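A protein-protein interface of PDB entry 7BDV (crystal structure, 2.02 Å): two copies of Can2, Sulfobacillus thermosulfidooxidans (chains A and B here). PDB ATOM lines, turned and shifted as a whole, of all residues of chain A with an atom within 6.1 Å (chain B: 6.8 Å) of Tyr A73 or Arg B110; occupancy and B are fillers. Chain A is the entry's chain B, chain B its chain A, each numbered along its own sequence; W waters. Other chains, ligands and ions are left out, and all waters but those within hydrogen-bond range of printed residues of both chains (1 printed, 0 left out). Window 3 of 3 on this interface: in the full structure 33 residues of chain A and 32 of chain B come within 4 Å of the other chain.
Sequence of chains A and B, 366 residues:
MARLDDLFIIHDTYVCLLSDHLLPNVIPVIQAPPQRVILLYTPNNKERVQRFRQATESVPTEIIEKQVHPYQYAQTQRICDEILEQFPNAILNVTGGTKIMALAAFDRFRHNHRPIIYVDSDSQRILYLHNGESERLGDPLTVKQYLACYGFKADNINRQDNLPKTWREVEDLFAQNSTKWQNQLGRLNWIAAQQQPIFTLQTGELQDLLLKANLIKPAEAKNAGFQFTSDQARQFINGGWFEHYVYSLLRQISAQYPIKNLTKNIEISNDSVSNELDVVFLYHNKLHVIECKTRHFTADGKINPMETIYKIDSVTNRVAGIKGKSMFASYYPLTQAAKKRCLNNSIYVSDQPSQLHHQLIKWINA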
ATOM      1  N   HIS A  69      30.509  10.620  13.617  1.00  0.00           N
ATOM      2  CA  HIS A  69      30.699  10.427  12.158  1.00  0.00           C
ATOM      3  C   HIS A  69      30.778  11.805  11.513  1.00  0.00           C
ATOM      4  O   HIS A  69      30.035  12.714  11.862  1.00  0.00           O
ATOM      5  CB  HIS A  69      29.623   9.514  11.567  1.00  0.00           C
ATOM      6  CG  HIS A  69      29.913   9.105  10.159  1.00  0.00           C
ATOM      7  ND1 HIS A  69      29.565   9.894   9.060  1.00  0.00           N
ATOM      8  CD2 HIS A  69      30.553   8.018   9.667  1.00  0.00           C
ATOM      9  CE1 HIS A  69      29.967   9.300   7.954  1.00  0.00           C
ATOM     10  NE2 HIS A  69      30.582   8.136   8.298  1.00  0.00           N
ATOM     11  N   TYR A  71      29.690  12.959   8.779  1.00  0.00           N
ATOM     12  CA  TYR A  71      28.583  13.303   7.842  1.00  0.00           C
ATOM     13  C   TYR A  71      27.230  12.806   8.330  1.00  0.00           C
ATOM     14  O   TYR A  71      26.375  12.528   7.486  1.00  0.00           O
ATOM     15  CB  TYR A  71      28.904  12.759   6.451  1.00  0.00           C
ATOM     16  CG  TYR A  71      30.166  13.338   5.885  1.00  0.00           C
ATOM     17  CD1 TYR A  71      30.221  14.666   5.479  1.00  0.00           C
ATOM     18  CD2 TYR A  71      31.328  12.578   5.796  1.00  0.00           C
ATOM     19  CE1 TYR A  71      31.387  15.214   4.973  1.00  0.00           C
ATOM     20  CE2 TYR A  71      32.505  13.135   5.335  1.00  0.00           C
ATOM     21  CZ  TYR A  71      32.530  14.448   4.901  1.00  0.00           C
ATOM     22  OH  TYR A  71      33.677  14.964   4.368  1.00  0.00           O
ATOM     23  N   GLN A  72      27.020  12.775   9.648  1.00  0.00           N
ATOM     24  CA  GLN A  72      25.781  12.317  10.314  1.00  0.00           C
ATOM     25  C   GLN A  72      25.288  13.422  11.249  1.00  0.00           C
ATOM     26  O   GLN A  72      25.745  13.487  12.449  1.00  0.00           O
ATOM     27  CB  GLN A  72      26.034  11.015  11.073  1.00  0.00           C
ATOM     28  CG  GLN A  72      25.869   9.774  10.214  1.00  0.00           C
ATOM     29  CD  GLN A  72      26.342   8.518  10.913  1.00  0.00           C
ATOM     30  OE1 GLN A  72      26.236   8.389  12.135  1.00  0.00           O
ATOM     31  NE2 GLN A  72      26.881   7.583  10.138  1.00  0.00           N
ATOM     32  N   TYR A  73      24.370  14.249  10.745  1.00  0.00           N
ATOM     33  CA  TYR A  73      23.792  15.422  11.451  1.00  0.00           C
ATOM     34  C   TYR A  73      23.219  15.000  12.806  1.00  0.00           C
ATOM     35  O   TYR A  73      23.665  15.528  13.845  1.00  0.00           O
ATOM     36  CB  TYR A  73      22.703  16.064  10.590  1.00  0.00           C
ATOM     37  CG  TYR A  73      22.195  17.385  11.102  1.00  0.00           C
ATOM     38  CD1 TYR A  73      22.975  18.524  11.033  1.00  0.00           C
ATOM     39  CD2 TYR A  73      20.908  17.512  11.589  1.00  0.00           C
ATOM     40  CE1 TYR A  73      22.503  19.756  11.470  1.00  0.00           C
ATOM     41  CE2 TYR A  73      20.417  18.727  12.041  1.00  0.00           C
ATOM     42  CZ  TYR A  73      21.222  19.852  12.001  1.00  0.00           C
ATOM     43  OH  TYR A  73      20.758  21.063  12.442  1.00  0.00           O
ATOM     44  N   ALA A  74      22.255  14.072  12.774  1.00  0.00           N
ATOM     45  CA  ALA A  74      21.460  13.553  13.912  1.00  0.00           C
ATOM     46  C   ALA A  74      22.359  12.984  15.012  1.00  0.00           C
ATOM     47  O   ALA A  74      22.099  13.263  16.189  1.00  0.00           O
ATOM     48  CB  ALA A  74      20.513  12.507  13.409  1.00  0.00           C
ATOM     49  N   GLN A  75      23.373  12.215  14.658  1.00  0.00           N
ATOM     50  CA  GLN A  75      24.285  11.576  15.647  1.00  0.00           C
ATOM     51  C   GLN A  75      25.113  12.657  16.359  1.00  0.00           C
ATOM     52  O   GLN A  75      25.383  12.508  17.556  1.00  0.00           O
ATOM     53  CB  GLN A  75      25.167  10.530  14.958  1.00  0.00           C
ATOM     54  CG  GLN A  75      26.091   9.795  15.923  1.00  0.00           C
ATOM     55  CD  GLN A  75      27.411   9.401  15.311  1.00  0.00           C
ATOM     56  OE1 GLN A  75      27.585   9.337  14.097  1.00  0.00           O
ATOM     57  NE2 GLN A  75      28.366   9.105  16.171  1.00  0.00           N
ATOM     58  N   THR A  76      25.510  13.719  15.667  1.00  0.00           N
ATOM     59  CA  THR A  76      26.290  14.818  16.287  1.00  0.00           C
ATOM     60  C   THR A  76      25.364  15.593  17.232  1.00  0.00           C
ATOM     61  O   THR A  76      25.829  15.954  18.359  1.00  0.00           O
ATOM     62  CB  THR A  76      27.008  15.673  15.239  1.00  0.00           C
ATOM     63  OG1 THR A  76      27.845  14.785  14.504  1.00  0.00           O
ATOM     64  CG2 THR A  76      27.805  16.808  15.856  1.00  0.00           C
ATOM     65  N   GLN A  77      24.107  15.803  16.823  1.00  0.00           N
ATOM     66  CA  GLN A  77      23.069  16.450  17.661  1.00  0.00           C
ATOM     67  C   GLN A  77      22.898  15.656  18.978  1.00  0.00           C
ATOM     68  O   GLN A  77      22.788  16.297  20.063  1.00  0.00           O
ATOM     69  CB  GLN A  77      21.743  16.537  16.917  1.00  0.00           C
ATOM     70  CG  GLN A  77      21.680  17.677  15.916  1.00  0.00           C
ATOM     71  CD  GLN A  77      20.336  17.715  15.229  1.00  0.00           C
ATOM     72  OE1 GLN A  77      19.915  16.724  14.627  1.00  0.00           O
ATOM     73  NE2 GLN A  77      19.680  18.872  15.289  1.00  0.00           N
ATOM     74  N   ARG A  78      22.884  14.328  18.889  1.00  0.00           N
ATOM     75  CA  ARG A  78      22.688  13.439  20.063  1.00  0.00           C
ATOM     76  C   ARG A  78      23.889  13.550  20.999  1.00  0.00           C
ATOM     77  O   ARG A  78      23.664  13.601  22.218  1.00  0.00           O
ATOM     78  CB  ARG A  78      22.446  11.989  19.648  1.00  0.00           C
ATOM     79  CG  ARG A  78      22.081  11.109  20.834  1.00  0.00           C
ATOM     80  CD  ARG A  78      21.741   9.703  20.418  1.00  0.00           C
ATOM     81  NE  ARG A  78      22.785   9.141  19.592  1.00  0.00           N
ATOM     82  CZ  ARG A  78      23.963   8.695  20.026  1.00  0.00           C
ATOM     83  NH1 ARG A  78      24.266   8.743  21.315  1.00  0.00           N
ATOM     84  NH2 ARG A  78      24.836   8.200  19.159  1.00  0.00           N
ATOM     85  N   ILE A 100      28.748  19.652   8.575  1.00  0.00           N
ATOM     86  CA  ILE A 100      27.676  18.811   9.178  1.00  0.00           C
ATOM     87  C   ILE A 100      27.896  18.799  10.700  1.00  0.00           C
ATOM     88  O   ILE A 100      26.992  19.113  11.459  1.00  0.00           O
ATOM     89  CB  ILE A 100      27.653  17.416   8.529  1.00  0.00           C
ATOM     90  CG1 ILE A 100      27.246  17.445   7.049  1.00  0.00           C
ATOM     91  CG2 ILE A 100      26.806  16.441   9.309  1.00  0.00           C
ATOM     92  CD1 ILE A 100      25.789  17.580   6.818  1.00  0.00           C
ATOM     93  N   LEU A 103      27.297  22.441  12.027  1.00  0.00           N
ATOM     94  CA  LEU A 103      25.851  22.837  12.019  1.00  0.00           C
ATOM     95  C   LEU A 103      25.106  22.122  13.165  1.00  0.00           C
ATOM     96  O   LEU A 103      24.284  22.769  13.839  1.00  0.00           O
ATOM     97  CB  LEU A 103      25.224  22.492  10.670  1.00  0.00           C
ATOM     98  CG  LEU A 103      25.676  23.358   9.490  1.00  0.00           C
ATOM     99  CD1 LEU A 103      25.253  22.726   8.180  1.00  0.00           C
ATOM    100  CD2 LEU A 103      25.090  24.752   9.584  1.00  0.00           C
ATOM    101  N   ALA A 104      25.355  20.833  13.352  1.00  0.00           N
ATOM    102  CA  ALA A 104      24.690  19.995  14.377  1.00  0.00           C
ATOM    103  C   ALA A 104      24.962  20.570  15.764  1.00  0.00           C
ATOM    104  O   ALA A 104      24.017  20.741  16.531  1.00  0.00           O
ATOM    105  CB  ALA A 104      25.212  18.583  14.285  1.00  0.00           C
ATOM    106  N   ALA A 105      26.228  20.846  16.069  1.00  0.00           N
ATOM    107  CA  ALA A 105      26.690  21.275  17.412  1.00  0.00           C
ATOM    108  C   ALA A 105      26.195  22.701  17.663  1.00  0.00           C
ATOM    109  O   ALA A 105      25.676  22.971  18.731  1.00  0.00           O
ATOM    110  CB  ALA A 105      28.189  21.172  17.488  1.00  0.00           C
ATOM    111  N   ASP A 107      23.515  24.129  16.470  1.00  0.00           N
ATOM    112  CA  ASP A 107      22.050  24.002  16.695  1.00  0.00           C
ATOM    113  C   ASP A 107      21.734  23.686  18.177  1.00  0.00           C
ATOM    114  O   ASP A 107      20.842  24.328  18.732  1.00  0.00           O
ATOM    115  CB  ASP A 107      21.486  22.915  15.783  1.00  0.00           C
ATOM    116  CG  ASP A 107      19.991  22.739  15.916  1.00  0.00           C
ATOM    117  OD1 ASP A 107      19.264  23.561  15.335  1.00  0.00           O
ATOM    118  OD2 ASP A 107      19.568  21.794  16.608  1.00  0.00           O
ATOM    119  N   ARG A 110      23.047  26.538  20.599  1.00  0.00           N
ATOM    120  CA  ARG A 110      22.171  27.726  20.438  1.00  0.00           C
ATOM    121  C   ARG A 110      20.873  27.473  21.209  1.00  0.00           C
ATOM    122  O   ARG A 110      20.468  28.344  22.009  1.00  0.00           O
ATOM    123  CB  ARG A 110      21.891  28.025  18.962  1.00  0.00           C
ATOM    124  CG  ARG A 110      21.092  29.305  18.744  1.00  0.00           C
ATOM    125  CD  ARG A 110      20.636  29.495  17.300  1.00  0.00           C
ATOM    126  NE  ARG A 110      19.673  28.477  16.894  1.00  0.00           N
ATOM    127  N   LEU B  84      15.249  35.058  -0.029  1.00  0.00           N
ATOM    128  CA  LEU B  84      14.043  34.240   0.251  1.00  0.00           C
ATOM    129  C   LEU B  84      12.761  35.064   0.060  1.00  0.00           C
ATOM    130  O   LEU B  84      11.721  34.465  -0.252  1.00  0.00           O
ATOM    131  CB  LEU B  84      14.154  33.666   1.666  1.00  0.00           C
ATOM    132  CG  LEU B  84      15.157  32.513   1.792  1.00  0.00           C
ATOM    133  CD1 LEU B  84      15.418  32.161   3.245  1.00  0.00           C
ATOM    134  CD2 LEU B  84      14.663  31.288   1.048  1.00  0.00           C
ATOM    135  N   LEU B  92      19.142  25.692  -0.922  1.00  0.00           N
ATOM    136  CA  LEU B  92      20.506  26.061  -0.461  1.00  0.00           C
ATOM    137  C   LEU B  92      21.415  24.843  -0.595  1.00  0.00           C
ATOM    138  O   LEU B  92      21.066  23.770  -0.089  1.00  0.00           O
ATOM    139  CB  LEU B  92      20.468  26.551   0.984  1.00  0.00           C
ATOM    140  CG  LEU B  92      21.833  26.851   1.600  1.00  0.00           C
ATOM    141  CD1 LEU B  92      22.427  28.087   0.975  1.00  0.00           C
ATOM    142  CD2 LEU B  92      21.731  27.039   3.108  1.00  0.00           C
ATOM    143  N   ALA B 105      23.295  31.091   6.519  1.00  0.00           N
ATOM    144  CA  ALA B 105      22.398  30.705   5.406  1.00  0.00           C
ATOM    145  C   ALA B 105      21.547  29.521   5.847  1.00  0.00           C
ATOM    146  O   ALA B 105      20.343  29.543   5.650  1.00  0.00           O
ATOM    147  CB  ALA B 105      23.220  30.422   4.168  1.00  0.00           C
ATOM    148  N   PHE B 106      22.155  28.502   6.455  1.00  0.00           N
ATOM    149  CA  PHE B 106      21.414  27.354   7.020  1.00  0.00           C
ATOM    150  C   PHE B 106      20.274  27.860   7.904  1.00  0.00           C
ATOM    151  O   PHE B 106      19.106  27.450   7.690  1.00  0.00           O
ATOM    152  CB  PHE B 106      22.352  26.440   7.805  1.00  0.00           C
ATOM    153  CG  PHE B 106      21.710  25.159   8.228  1.00  0.00           C
ATOM    154  CD1 PHE B 106      21.619  24.084   7.356  1.00  0.00           C
ATOM    155  CD2 PHE B 106      21.233  25.012   9.512  1.00  0.00           C
ATOM    156  CE1 PHE B 106      21.063  22.885   7.773  1.00  0.00           C
ATOM    157  CE2 PHE B 106      20.705  23.800   9.937  1.00  0.00           C
ATOM    158  CZ  PHE B 106      20.605  22.745   9.063  1.00  0.00           C
ATOM    159  N   ASP B 107      20.595  28.726   8.867  1.00  0.00           N
ATOM    160  CA  ASP B 107      19.631  29.271   9.855  1.00  0.00           C
ATOM    161  C   ASP B 107      18.379  29.842   9.160  1.00  0.00           C
ATOM    162  O   ASP B 107      17.267  29.518   9.602  1.00  0.00           O
ATOM    163  CB  ASP B 107      20.289  30.341  10.728  1.00  0.00           C
ATOM    164  CG  ASP B 107      19.355  30.858  11.810  1.00  0.00           C
ATOM    165  OD1 ASP B 107      19.189  30.157  12.831  1.00  0.00           O
ATOM    166  OD2 ASP B 107      18.771  31.956  11.611  1.00  0.00           O
ATOM    167  N   ARG B 108      18.542  30.683   8.140  1.00  0.00           N
ATOM    168  CA  ARG B 108      17.410  31.384   7.470  1.00  0.00           C
ATOM    169  C   ARG B 108      16.651  30.411   6.560  1.00  0.00           C
ATOM    170  O   ARG B 108      15.423  30.531   6.473  1.00  0.00           O
ATOM    171  CB  ARG B 108      17.901  32.575   6.647  1.00  0.00           C
ATOM    172  CG  ARG B 108      18.659  33.622   7.445  1.00  0.00           C
ATOM    173  CD  ARG B 108      18.115  33.842   8.849  1.00  0.00           C
ATOM    174  NE  ARG B 108      16.731  34.277   8.809  1.00  0.00           N
ATOM    175  CZ  ARG B 108      15.859  34.169   9.806  1.00  0.00           C
ATOM    176  NH1 ARG B 108      16.202  33.606  10.956  1.00  0.00           N
ATOM    177  NH2 ARG B 108      14.627  34.617   9.641  1.00  0.00           N
ATOM    178  N   PHE B 109      17.349  29.472   5.914  1.00  0.00           N
ATOM    179  CA  PHE B 109      16.725  28.462   5.028  1.00  0.00           C
ATOM    180  C   PHE B 109      15.953  27.447   5.878  1.00  0.00           C
ATOM    181  O   PHE B 109      14.858  27.037   5.460  1.00  0.00           O
ATOM    182  CB  PHE B 109      17.761  27.844   4.094  1.00  0.00           C
ATOM    183  CG  PHE B 109      17.970  28.635   2.832  1.00  0.00           C
ATOM    184  CD1 PHE B 109      18.726  29.784   2.838  1.00  0.00           C
ATOM    185  CD2 PHE B 109      17.432  28.198   1.639  1.00  0.00           C
ATOM    186  CE1 PHE B 109      18.928  30.507   1.667  1.00  0.00           C
ATOM    187  CE2 PHE B 109      17.612  28.924   0.475  1.00  0.00           C
ATOM    188  CZ  PHE B 109      18.372  30.064   0.488  1.00  0.00           C
ATOM    189  N   ARG B 110      16.465  27.087   7.052  1.00  0.00           N
ATOM    190  CA  ARG B 110      15.749  26.180   7.986  1.00  0.00           C
ATOM    191  C   ARG B 110      14.484  26.894   8.503  1.00  0.00           C
ATOM    192  O   ARG B 110      13.380  26.292   8.465  1.00  0.00           O
ATOM    193  CB  ARG B 110      16.654  25.755   9.143  1.00  0.00           C
ATOM    194  CG  ARG B 110      16.009  24.746  10.082  1.00  0.00           C
ATOM    195  CD  ARG B 110      16.918  24.288  11.211  1.00  0.00           C
ATOM    196  NE  ARG B 110      17.220  25.395  12.108  1.00  0.00           N
ATOM    197  CZ  ARG B 110      18.269  25.455  12.926  1.00  0.00           C
ATOM    198  NH1 ARG B 110      19.129  24.451  12.996  1.00  0.00           N
ATOM    199  NH2 ARG B 110      18.451  26.532  13.675  1.00  0.00           N
ATOM    200  N   HIS B 111      14.620  28.139   8.957  1.00  0.00           N
ATOM    201  CA  HIS B 111      13.496  28.955   9.483  1.00  0.00           C
ATOM    202  C   HIS B 111      12.352  29.019   8.454  1.00  0.00           C
ATOM    203  O   HIS B 111      11.192  29.007   8.880  1.00  0.00           O
ATOM    204  CB  HIS B 111      13.991  30.338   9.918  1.00  0.00           C
ATOM    205  CG  HIS B 111      12.901  31.206  10.446  1.00  0.00           C
ATOM    206  ND1 HIS B 111      12.495  31.165  11.772  1.00  0.00           N
ATOM    207  CD2 HIS B 111      12.132  32.140   9.839  1.00  0.00           C
ATOM    208  CE1 HIS B 111      11.513  32.026  11.949  1.00  0.00           C
ATOM    209  NE2 HIS B 111      11.280  32.645  10.782  1.00  0.00           N
ATOM    210  N   ASN B 112      12.666  29.074   7.158  1.00  0.00           N
ATOM    211  CA  ASN B 112      11.676  29.150   6.045  1.00  0.00           C
ATOM    212  C   ASN B 112      11.350  27.768   5.473  1.00  0.00           C
ATOM    213  O   ASN B 112      10.827  27.729   4.361  1.00  0.00           O
ATOM    214  CB  ASN B 112      12.166  30.055   4.920  1.00  0.00           C
ATOM    215  CG  ASN B 112      12.129  31.520   5.276  1.00  0.00           C
ATOM    216  OD1 ASN B 112      11.186  32.217   4.915  1.00  0.00           O
ATOM    217  ND2 ASN B 112      13.108  31.986   6.034  1.00  0.00           N
ATOM    218  N   HIS B 113      11.654  26.681   6.194  1.00  0.00           N
ATOM    219  CA  HIS B 113      11.347  25.280   5.803  1.00  0.00           C
ATOM    220  C   HIS B 113      11.753  25.011   4.347  1.00  0.00           C
ATOM    221  O   HIS B 113      10.957  24.388   3.607  1.00  0.00           O
ATOM    222  CB  HIS B 113       9.860  24.970   6.070  1.00  0.00           C
ATOM    223  CG  HIS B 113       9.494  25.161   7.502  1.00  0.00           C
ATOM    224  ND1 HIS B 113       9.031  26.374   7.984  1.00  0.00           N
ATOM    225  CD2 HIS B 113       9.575  24.325   8.567  1.00  0.00           C
ATOM    226  CE1 HIS B 113       8.828  26.276   9.287  1.00  0.00           C
ATOM    227  NE2 HIS B 113       9.163  25.026   9.671  1.00  0.00           N
ATOM    228  N   ARG B 114      12.954  25.443   3.959  1.00  0.00           N
ATOM    229  CA  ARG B 114      13.495  25.264   2.588  1.00  0.00           C
ATOM    230  C   ARG B 114      14.361  24.008   2.536  1.00  0.00           C
ATOM    231  O   ARG B 114      14.950  23.602   3.541  1.00  0.00           O
ATOM    232  CB  ARG B 114      14.312  26.483   2.164  1.00  0.00           C
ATOM    233  CG  ARG B 114      13.580  27.817   2.190  1.00  0.00           C
ATOM    234  CD  ARG B 114      12.251  27.859   1.448  1.00  0.00           C
ATOM    235  NE  ARG B 114      12.330  27.273   0.132  1.00  0.00           N
ATOM    236  CZ  ARG B 114      11.423  26.496  -0.439  1.00  0.00           C
ATOM    237  NH1 ARG B 114      10.282  26.229   0.179  1.00  0.00           N
ATOM    238  NH2 ARG B 114      11.664  26.050  -1.658  1.00  0.00           N
ATOM    239  N   ILE B 116      17.699  21.953   1.841  1.00  0.00           N
ATOM    240  CA  ILE B 116      19.138  22.248   2.063  1.00  0.00           C
ATOM    241  C   ILE B 116      19.911  20.973   1.748  1.00  0.00           C
ATOM    242  O   ILE B 116      19.646  19.954   2.391  1.00  0.00           O
ATOM    243  CB  ILE B 116      19.420  22.747   3.492  1.00  0.00           C
ATOM    244  CG1 ILE B 116      18.603  23.984   3.847  1.00  0.00           C
ATOM    245  CG2 ILE B 116      20.915  23.012   3.639  1.00  0.00           C
ATOM    246  CD1 ILE B 116      18.587  24.318   5.347  1.00  0.00           C
ATOM    247  N   LEU B 127      23.414  14.765   0.681  1.00  0.00           N
ATOM    248  CA  LEU B 127      22.597  14.700   1.918  1.00  0.00           C
ATOM    249  C   LEU B 127      21.543  15.808   1.846  1.00  0.00           C
ATOM    250  O   LEU B 127      21.913  16.931   1.554  1.00  0.00           O
ATOM    251  CB  LEU B 127      23.485  14.877   3.149  1.00  0.00           C
ATOM    252  CG  LEU B 127      24.748  14.028   3.168  1.00  0.00           C
ATOM    253  CD1 LEU B 127      25.493  14.228   4.484  1.00  0.00           C
ATOM    254  CD2 LEU B 127      24.414  12.580   2.940  1.00  0.00           C
ATOM    255  N   LEU B 129      19.536  17.802   4.190  1.00  0.00           N
ATOM    256  CA  LEU B 129      19.657  18.114   5.638  1.00  0.00           C
ATOM    257  C   LEU B 129      18.291  18.459   6.220  1.00  0.00           C
ATOM    258  O   LEU B 129      18.130  18.294   7.424  1.00  0.00           O
ATOM    259  CB  LEU B 129      20.665  19.250   5.836  1.00  0.00           C
ATOM    260  CG  LEU B 129      22.112  18.854   5.547  1.00  0.00           C
ATOM    261  CD1 LEU B 129      23.083  19.947   5.961  1.00  0.00           C
ATOM    262  CD2 LEU B 129      22.478  17.553   6.253  1.00  0.00           C
HETATM  263  O   HOH W   1      22.511  24.982  12.991  1.00  0.00           O
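NH1 of Arg B110 lies within salt-bridge range of OD1 of Asp A107.
OD1 of Asp B107 lies within salt-bridge range of NH2 of Arg B110 (3.8 Å).
O of Ile B116 lies within hydrogen-bond range of N of Leu B129 (2.8 Å).
N of Tyr A71 sits at hydrogen-bond distance from ND1 of His A69, 3.1 Å away.
NE2 of Gln A77 lies within hydrogen-bond range of OD2 of Asp A107 (3.2 Å).
Among the printed residues, merely in contact across the chains: Tyr A71 with Leu B127 (3.6 Å), Tyr A73 with Phe B106 (3.7 Å), Tyr A73 with Arg B110 (3.8 Å), Ile A100 with Leu B129 (3.4 Å), Leu A103 with Phe B106 (3.7 Å) and Arg A110 with Arg B110 (3.95 Å).
Tyr A73 touches just these residues of chain B: Phe B106 (3.7 Å) and Arg B110 (3.8 Å).
Of the printed residues of chain B, Ile A100 touches Leu B129.
Of the printed residues of chain B, Leu A103 touches Phe B106 (3.7 Å).
Of the printed residues of chain B, Asp A107 touches Arg B110 (2.5 Å).
Of the printed residues of chain B, Arg A110 touches Arg B110 (3.95 Å).
The nearest printed residue of chain B that does not touch Arg A110 is Asp B107 (4.4 Å).
Printed residues of chain A that touch a printed residue of chain B: Tyr A71, Tyr A73, Ile A100, Leu A103, Asp A107 and Arg A110.
Printed residues of chain B that touch a printed residue of chain A: Phe B106, Arg B110, Leu B127 and Leu B129.
Among the printed residues, 7 pairs touch across the chains.
Asp A107 touches Arg B110, but with the chains exchanged Arg A110 does not touch Asp B107 (4.4 Å).
Arg B110 touches its own counterpart, Arg A110.
Positions printed for both chains: 105, 107 and 110.
Water W1 lies within hydrogen-bond range of the backbone carbonyl oxygen (O) of Leu A103 (3.0 Å) and the guanidinium group (NH1) of Arg B110 (3.4 Å).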
